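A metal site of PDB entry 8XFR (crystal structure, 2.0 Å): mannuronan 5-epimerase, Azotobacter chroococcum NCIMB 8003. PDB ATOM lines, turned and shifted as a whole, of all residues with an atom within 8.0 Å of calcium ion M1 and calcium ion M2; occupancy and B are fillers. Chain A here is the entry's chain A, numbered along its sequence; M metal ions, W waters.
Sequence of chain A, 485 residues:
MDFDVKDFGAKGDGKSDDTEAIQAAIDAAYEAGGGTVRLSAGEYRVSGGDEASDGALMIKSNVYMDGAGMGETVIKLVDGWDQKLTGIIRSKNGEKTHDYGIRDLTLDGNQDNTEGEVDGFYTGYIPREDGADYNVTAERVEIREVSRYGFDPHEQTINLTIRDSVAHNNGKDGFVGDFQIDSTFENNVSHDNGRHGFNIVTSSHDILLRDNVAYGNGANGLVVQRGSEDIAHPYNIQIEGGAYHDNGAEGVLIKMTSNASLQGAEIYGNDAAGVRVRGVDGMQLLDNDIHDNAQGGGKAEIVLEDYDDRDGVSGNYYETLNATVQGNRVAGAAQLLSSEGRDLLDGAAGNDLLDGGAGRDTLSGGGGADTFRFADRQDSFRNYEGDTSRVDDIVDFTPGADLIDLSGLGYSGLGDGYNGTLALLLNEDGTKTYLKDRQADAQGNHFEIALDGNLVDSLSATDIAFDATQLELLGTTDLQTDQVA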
ATOM      1  N   VAL A 330     -17.919   4.704 -29.010  1.00  0.00           N
ATOM      2  CA  VAL A 330     -18.164   3.582 -29.918  1.00  0.00           C
ATOM      3  C   VAL A 330     -19.554   3.068 -29.610  1.00  0.00           C
ATOM      4  O   VAL A 330     -19.777   2.462 -28.553  1.00  0.00           O
ATOM      5  CB  VAL A 330     -17.136   2.448 -29.794  1.00  0.00           C
ATOM      6  CG1 VAL A 330     -17.287   1.451 -30.958  1.00  0.00           C
ATOM      7  CG2 VAL A 330     -15.718   3.003 -29.785  1.00  0.00           C
ATOM      8  N   GLY A 332     -21.444   0.517 -30.279  1.00  0.00           N
ATOM      9  CA  GLY A 332     -21.459  -0.849 -30.764  1.00  0.00           C
ATOM     10  C   GLY A 332     -20.224  -1.559 -30.250  1.00  0.00           C
ATOM     11  O   GLY A 332     -19.422  -1.001 -29.504  1.00  0.00           O
ATOM     12  N   ALA A 333     -20.085  -2.814 -30.668  1.00  0.00           N
ATOM     13  CA  ALA A 333     -19.115  -3.691 -30.026  1.00  0.00           C
ATOM     14  C   ALA A 333     -17.710  -3.494 -30.569  1.00  0.00           C
ATOM     15  O   ALA A 333     -17.487  -3.391 -31.787  1.00  0.00           O
ATOM     16  CB  ALA A 333     -19.535  -5.149 -30.201  1.00  0.00           C
ATOM     17  N   ALA A 334     -16.733  -3.491 -29.664  1.00  0.00           N
ATOM     18  CA  ALA A 334     -15.316  -3.404 -30.032  1.00  0.00           C
ATOM     19  C   ALA A 334     -14.645  -4.732 -29.722  1.00  0.00           C
ATOM     20  O   ALA A 334     -14.738  -5.226 -28.591  1.00  0.00           O
ATOM     21  CB  ALA A 334     -14.620  -2.265 -29.280  1.00  0.00           C
ATOM     22  N   ASP A 346      -9.323  -0.052 -23.948  1.00  0.00           N
ATOM     23  CA  ASP A 346     -10.522   0.477 -23.315  1.00  0.00           C
ATOM     24  C   ASP A 346     -11.664   0.255 -24.292  1.00  0.00           C
ATOM     25  O   ASP A 346     -11.611   0.756 -25.416  1.00  0.00           O
ATOM     26  CB  ASP A 346     -10.386   1.986 -23.017  1.00  0.00           C
ATOM     27  CG  ASP A 346      -9.345   2.299 -21.948  1.00  0.00           C
ATOM     28  OD1 ASP A 346      -9.007   3.496 -21.821  1.00  0.00           O
ATOM     29  OD2 ASP A 346      -8.870   1.370 -21.214  1.00  0.00           O
ATOM     30  N   GLY A 347     -12.689  -0.475 -23.853  1.00  0.00           N
ATOM     31  CA  GLY A 347     -13.921  -0.529 -24.609  1.00  0.00           C
ATOM     32  C   GLY A 347     -14.751   0.734 -24.375  1.00  0.00           C
ATOM     33  O   GLY A 347     -14.336   1.670 -23.688  1.00  0.00           O
ATOM     34  N   ALA A 348     -15.954   0.750 -24.923  1.00  0.00           N
ATOM     35  CA  ALA A 348     -16.865   1.907 -24.846  1.00  0.00           C
ATOM     36  C   ALA A 348     -18.261   1.356 -24.581  1.00  0.00           C
ATOM     37  O   ALA A 348     -18.433   0.366 -23.862  1.00  0.00           O
ATOM     38  CB  ALA A 348     -16.753   2.815 -26.077  1.00  0.00           C
ATOM     39  N   ALA A 349     -19.299   2.084 -25.028  1.00  0.00           N
ATOM     40  CA  ALA A 349     -20.680   1.775 -24.656  1.00  0.00           C
ATOM     41  C   ALA A 349     -21.135   0.378 -25.072  1.00  0.00           C
ATOM     42  O   ALA A 349     -22.116  -0.136 -24.509  1.00  0.00           O
ATOM     43  CB  ALA A 349     -21.632   2.830 -25.251  1.00  0.00           C
ATOM     44  N   GLY A 350     -20.475  -0.264 -26.036  1.00  0.00           N
ATOM     45  CA  GLY A 350     -20.927  -1.550 -26.534  1.00  0.00           C
ATOM     46  C   GLY A 350     -20.530  -2.713 -25.628  1.00  0.00           C
ATOM     47  O   GLY A 350     -19.872  -2.563 -24.606  1.00  0.00           O
ATOM     48  N   ASN A 351     -20.962  -3.914 -26.031  1.00  0.00           N
ATOM     49  CA  ASN A 351     -20.628  -5.155 -25.342  1.00  0.00           C
ATOM     50  C   ASN A 351     -19.348  -5.680 -25.980  1.00  0.00           C
ATOM     51  O   ASN A 351     -19.389  -6.337 -27.009  1.00  0.00           O
ATOM     52  CB  ASN A 351     -21.746  -6.190 -25.470  1.00  0.00           C
ATOM     53  CG  ASN A 351     -22.944  -5.879 -24.602  1.00  0.00           C
ATOM     54  OD1 ASN A 351     -23.004  -4.871 -23.895  1.00  0.00           O
ATOM     55  ND2 ASN A 351     -23.904  -6.776 -24.630  1.00  0.00           N
ATOM     56  N   ASP A 352     -18.211  -5.367 -25.368  1.00  0.00           N
ATOM     57  CA  ASP A 352     -16.912  -5.538 -25.993  1.00  0.00           C
ATOM     58  C   ASP A 352     -16.213  -6.816 -25.552  1.00  0.00           C
ATOM     59  O   ASP A 352     -16.472  -7.363 -24.470  1.00  0.00           O
ATOM     60  CB  ASP A 352     -16.022  -4.326 -25.697  1.00  0.00           C
ATOM     61  CG  ASP A 352     -16.742  -3.004 -25.937  1.00  0.00           C
ATOM     62  OD1 ASP A 352     -17.340  -2.839 -27.017  1.00  0.00           O
ATOM     63  OD2 ASP A 352     -16.695  -2.129 -25.056  1.00  0.00           O
ATOM     64  N   LEU A 353     -15.297  -7.282 -26.397  1.00  0.00           N
ATOM     65  CA  LEU A 353     -14.406  -8.404 -26.088  1.00  0.00           C
ATOM     66  C   LEU A 353     -12.990  -7.866 -25.982  1.00  0.00           C
ATOM     67  O   LEU A 353     -12.486  -7.283 -26.949  1.00  0.00           O
ATOM     68  CB  LEU A 353     -14.478  -9.484 -27.178  1.00  0.00           C
ATOM     69  CG  LEU A 353     -13.449 -10.610 -27.096  1.00  0.00           C
ATOM     70  CD1 LEU A 353     -13.667 -11.438 -25.847  1.00  0.00           C
ATOM     71  CD2 LEU A 353     -13.461 -11.533 -28.321  1.00  0.00           C
ATOM     72  N   LEU A 354     -12.336  -8.088 -24.838  1.00  0.00           N
ATOM     73  CA  LEU A 354     -11.002  -7.567 -24.594  1.00  0.00           C
ATOM     74  C   LEU A 354     -10.037  -8.690 -24.268  1.00  0.00           C
ATOM     75  O   LEU A 354     -10.318  -9.526 -23.403  1.00  0.00           O
ATOM     76  CB  LEU A 354     -10.997  -6.550 -23.438  1.00  0.00           C
ATOM     77  CG  LEU A 354     -11.811  -5.315 -23.840  1.00  0.00           C
ATOM     78  CD1 LEU A 354     -13.177  -5.400 -23.197  1.00  0.00           C
ATOM     79  CD2 LEU A 354     -11.077  -4.069 -23.398  1.00  0.00           C
ATOM     80  N   SER A 364     -10.167  -2.060 -19.779  1.00  0.00           N
ATOM     81  CA  SER A 364     -11.386  -1.550 -19.193  1.00  0.00           C
ATOM     82  C   SER A 364     -12.528  -1.772 -20.170  1.00  0.00           C
ATOM     83  O   SER A 364     -12.338  -1.731 -21.392  1.00  0.00           O
ATOM     84  CB  SER A 364     -11.253  -0.074 -18.836  1.00  0.00           C
ATOM     85  OG  SER A 364     -11.385   0.716 -20.001  1.00  0.00           O
ATOM     86  N   GLY A 365     -13.710  -2.049 -19.627  1.00  0.00           N
ATOM     87  CA  GLY A 365     -14.834  -2.318 -20.482  1.00  0.00           C
ATOM     88  C   GLY A 365     -15.653  -1.080 -20.841  1.00  0.00           C
ATOM     89  O   GLY A 365     -16.291  -1.059 -21.897  1.00  0.00           O
ATOM     90  N   GLY A 366     -15.669  -0.066 -19.959  1.00  0.00           N
ATOM     91  CA  GLY A 366     -16.653   0.974 -20.206  1.00  0.00           C
ATOM     92  C   GLY A 366     -18.073   0.467 -19.992  1.00  0.00           C
ATOM     93  O   GLY A 366     -18.312  -0.555 -19.331  1.00  0.00           O
ATOM     94  N   GLY A 367     -19.028   1.183 -20.590  1.00  0.00           N
ATOM     95  CA  GLY A 367     -20.430   0.831 -20.448  1.00  0.00           C
ATOM     96  C   GLY A 367     -20.716  -0.534 -21.055  1.00  0.00           C
ATOM     97  O   GLY A 367     -19.868  -1.151 -21.693  1.00  0.00           O
ATOM     98  N   GLY A 368     -21.917  -1.044 -20.806  1.00  0.00           N
ATOM     99  CA  GLY A 368     -22.306  -2.320 -21.372  1.00  0.00           C
ATOM    100  C   GLY A 368     -21.670  -3.532 -20.684  1.00  0.00           C
ATOM    101  O   GLY A 368     -20.947  -3.421 -19.688  1.00  0.00           O
ATOM    102  N   ALA A 369     -21.945  -4.700 -21.242  1.00  0.00           N
ATOM    103  CA  ALA A 369     -21.529  -5.962 -20.662  1.00  0.00           C
ATOM    104  C   ALA A 369     -20.333  -6.488 -21.453  1.00  0.00           C
ATOM    105  O   ALA A 369     -20.470  -6.912 -22.594  1.00  0.00           O
ATOM    106  CB  ALA A 369     -22.681  -6.962 -20.684  1.00  0.00           C
ATOM    107  N   ASP A 370     -19.161  -6.495 -20.824  1.00  0.00           N
ATOM    108  CA  ASP A 370     -17.909  -6.787 -21.515  1.00  0.00           C
ATOM    109  C   ASP A 370     -17.300  -8.080 -21.021  1.00  0.00           C
ATOM    110  O   ASP A 370     -17.380  -8.411 -19.825  1.00  0.00           O
ATOM    111  CB  ASP A 370     -16.931  -5.643 -21.343  1.00  0.00           C
ATOM    112  CG  ASP A 370     -17.533  -4.317 -21.766  1.00  0.00           C
ATOM    113  OD1 ASP A 370     -17.879  -4.153 -22.947  1.00  0.00           O
ATOM    114  OD2 ASP A 370     -17.694  -3.462 -20.902  1.00  0.00           O
ATOM    115  N   THR A 371     -16.688  -8.815 -21.959  1.00  0.00           N
ATOM    116  CA  THR A 371     -15.988 -10.054 -21.683  1.00  0.00           C
ATOM    117  C   THR A 371     -14.485  -9.769 -21.748  1.00  0.00           C
ATOM    118  O   THR A 371     -13.981  -9.293 -22.770  1.00  0.00           O
ATOM    119  CB  THR A 371     -16.372 -11.127 -22.702  1.00  0.00           C
ATOM    120  OG1 THR A 371     -17.755 -11.479 -22.523  1.00  0.00           O
ATOM    121  CG2 THR A 371     -15.527 -12.359 -22.514  1.00  0.00           C
ATOM    122  N   PHE A 372     -13.795 -10.028 -20.632  1.00  0.00           N
ATOM    123  CA  PHE A 372     -12.333  -9.988 -20.569  1.00  0.00           C
ATOM    124  C   PHE A 372     -11.827 -11.412 -20.690  1.00  0.00           C
ATOM    125  O   PHE A 372     -12.021 -12.228 -19.783  1.00  0.00           O
ATOM    126  CB  PHE A 372     -11.878  -9.334 -19.263  1.00  0.00           C
ATOM    127  CG  PHE A 372     -12.489  -7.981 -19.042  1.00  0.00           C
ATOM    128  CD1 PHE A 372     -13.711  -7.854 -18.387  1.00  0.00           C
ATOM    129  CD2 PHE A 372     -11.871  -6.839 -19.527  1.00  0.00           C
ATOM    130  CE1 PHE A 372     -14.289  -6.599 -18.211  1.00  0.00           C
ATOM    131  CE2 PHE A 372     -12.442  -5.583 -19.344  1.00  0.00           C
ATOM    132  CZ  PHE A 372     -13.661  -5.466 -18.690  1.00  0.00           C
ATOM    133  N   ASP A 396     -12.335  -1.659 -14.463  1.00  0.00           N
ATOM    134  CA  ASP A 396     -13.717  -1.307 -14.117  1.00  0.00           C
ATOM    135  C   ASP A 396     -14.632  -2.529 -14.150  1.00  0.00           C
ATOM    136  O   ASP A 396     -15.757  -2.465 -14.652  1.00  0.00           O
ATOM    137  CB  ASP A 396     -14.264  -0.228 -15.056  1.00  0.00           C
ATOM    138  CG  ASP A 396     -14.249  -0.677 -16.528  1.00  0.00           C
ATOM    139  OD1 ASP A 396     -13.583  -1.690 -16.845  1.00  0.00           O
ATOM    140  OD2 ASP A 396     -14.884   0.000 -17.375  1.00  0.00           O
ATOM    141  N   PHE A 397     -14.172  -3.651 -13.623  1.00  0.00           N
ATOM    142  CA  PHE A 397     -14.994  -4.845 -13.713  1.00  0.00           C
ATOM    143  C   PHE A 397     -16.299  -4.644 -12.954  1.00  0.00           C
ATOM    144  O   PHE A 397     -16.308  -4.203 -11.806  1.00  0.00           O
ATOM    145  CB  PHE A 397     -14.280  -6.084 -13.157  1.00  0.00           C
ATOM    146  CG  PHE A 397     -14.998  -7.345 -13.478  1.00  0.00           C
ATOM    147  CD1 PHE A 397     -14.844  -7.928 -14.711  1.00  0.00           C
ATOM    148  CD2 PHE A 397     -15.880  -7.906 -12.582  1.00  0.00           C
ATOM    149  CE1 PHE A 397     -15.526  -9.080 -15.049  1.00  0.00           C
ATOM    150  CE2 PHE A 397     -16.573  -9.053 -12.898  1.00  0.00           C
ATOM    151  CZ  PHE A 397     -16.402  -9.642 -14.131  1.00  0.00           C
ATOM    152  N   THR A 398     -17.407  -4.996 -13.601  1.00  0.00           N
ATOM    153  CA  THR A 398     -18.729  -4.759 -13.029  1.00  0.00           C
ATOM    154  C   THR A 398     -19.409  -6.089 -12.737  1.00  0.00           C
ATOM    155  O   THR A 398     -19.925  -6.740 -13.671  1.00  0.00           O
ATOM    156  CB  THR A 398     -19.572  -3.929 -13.978  1.00  0.00           C
ATOM    157  OG1 THR A 398     -18.821  -2.761 -14.368  1.00  0.00           O
ATOM    158  CG2 THR A 398     -20.858  -3.519 -13.296  1.00  0.00           C
ATOM    159  N   ALA A 401     -22.553  -7.692 -14.553  1.00  0.00           N
ATOM    160  CA  ALA A 401     -22.594  -7.178 -15.929  1.00  0.00           C
ATOM    161  C   ALA A 401     -21.476  -7.750 -16.780  1.00  0.00           C
ATOM    162  O   ALA A 401     -21.748  -8.370 -17.824  1.00  0.00           O
ATOM    163  CB  ALA A 401     -22.508  -5.647 -15.923  1.00  0.00           C
ATOM    164  N   ASP A 402     -20.231  -7.593 -16.365  1.00  0.00           N
ATOM    165  CA  ASP A 402     -19.095  -8.042 -17.152  1.00  0.00           C
ATOM    166  C   ASP A 402     -18.831  -9.530 -16.896  1.00  0.00           C
ATOM    167  O   ASP A 402     -19.413 -10.156 -16.003  1.00  0.00           O
ATOM    168  CB  ASP A 402     -17.851  -7.214 -16.819  1.00  0.00           C
ATOM    169  CG  ASP A 402     -18.021  -5.728 -17.145  1.00  0.00           C
ATOM    170  OD1 ASP A 402     -18.749  -5.380 -18.103  1.00  0.00           O
ATOM    171  OD2 ASP A 402     -17.382  -4.906 -16.443  1.00  0.00           O
ATOM    172  N   LEU A 403     -17.920 -10.091 -17.687  1.00  0.00           N
ATOM    173  CA  LEU A 403     -17.535 -11.496 -17.571  1.00  0.00           C
ATOM    174  C   LEU A 403     -16.038 -11.676 -17.783  1.00  0.00           C
ATOM    175  O   LEU A 403     -15.464 -11.106 -18.729  1.00  0.00           O
ATOM    176  CB  LEU A 403     -18.300 -12.359 -18.585  1.00  0.00           C
ATOM    177  CG  LEU A 403     -17.922 -13.829 -18.603  1.00  0.00           C
ATOM    178  CD1 LEU A 403     -18.487 -14.509 -17.360  1.00  0.00           C
ATOM    179  CD2 LEU A 403     -18.414 -14.485 -19.904  1.00  0.00           C
ATOM    180  N   THR A 476     -21.044 -12.397 -22.937  1.00  0.00           N
ATOM    181  CA  THR A 476     -21.739 -11.137 -23.073  1.00  0.00           C
ATOM    182  C   THR A 476     -21.729 -10.609 -24.495  1.00  0.00           C
ATOM    183  O   THR A 476     -22.445  -9.658 -24.793  1.00  0.00           O
ATOM    184  CB  THR A 476     -21.101 -10.099 -22.139  1.00  0.00           C
ATOM    185  OG1 THR A 476     -19.860  -9.639 -22.712  1.00  0.00           O
ATOM    186  CG2 THR A 476     -20.868 -10.695 -20.736  1.00  0.00           C
HETATM  187 CA    CA M   1     -18.092  -1.793 -23.191  1.00  0.00          CA
HETATM  188 CA    CA M   2     -18.750  -2.870 -18.788  1.00  0.00          CA
HETATM  189  O   HOH W   1     -19.722  -2.032 -16.600  1.00  0.00           O
HETATM  190  O   HOH W   2     -16.391  -2.929 -17.553  1.00  0.00           O
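Within 4 Å of calcium ion M1: Ala 348, Gly 350, Asp 352, Gly 365, Gly 366, Gly 367 and Asp 370.
Water W2 lies within hydrogen-bond range of OD2 of Asp 402 (2.5 Å) and O of Asp 396 (3.0 Å).
O of Ala 348 binds calcium ion M1 (2.3 Å).
O of Gly 365 binds calcium ion M1.
OD2 of Asp 352 binds calcium ion M1 (2.4 Å).
The side-chain carboxylate (OD1) of Asp 370 binds calcium ion M1 (2.4 Å).
O of Gly 350 is bound to calcium ion M1, 2.4 Å away.
O of Gly 367 binds calcium ion M1, 2.4 Å away.
The side-chain carboxylate (OD2) of Asp 370 is bound to calcium ion M1 (2.9 Å).
Calcium ion M1 has seven donor atoms within binding distance.
The nearest printed residue that does not touch calcium ion M2 is Gly 365 (4.1 Å).
N of Thr 371 sits at hydrogen-bond distance from O of Asp 352.
The side-chain carboxylate of Asp 352 sits at hydrogen-bond distance from the backbone NH of Ala 334 (2.8 Å).
The side-chain carboxylate (OD2) of Asp 402 lies within hydrogen-bond range of the backbone NH (N) of Thr 398.
O of Asp 370 is in hydrogen-bond range of N of Leu 403 (2.8 Å).
The side-chain carboxylate of Asp 396 lies within hydrogen-bond range of the backbone NH of Gly 366 (2.7 Å).
The side-chain carboxylate (OD1) of Asp 396 lies within hydrogen-bond range of the backbone NH (N) of Gly 365, 2.8 Å away.
O of Gly 366 binds calcium ion M2, at 2.4 Å.
Calcium ion M2 is bound by the side-chain carboxylate (OD2) of Asp 370, at 2.4 Å.
Calcium ion M2 is bound by O of Gly 368, at 2.4 Å.
Calcium ion M2 is bound by water W1, 2.5 Å away.
Calcium ion M2 is bound by OD1 of Asp 402 (2.6 Å).
Water W2 binds calcium ion M2, at 2.7 Å.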
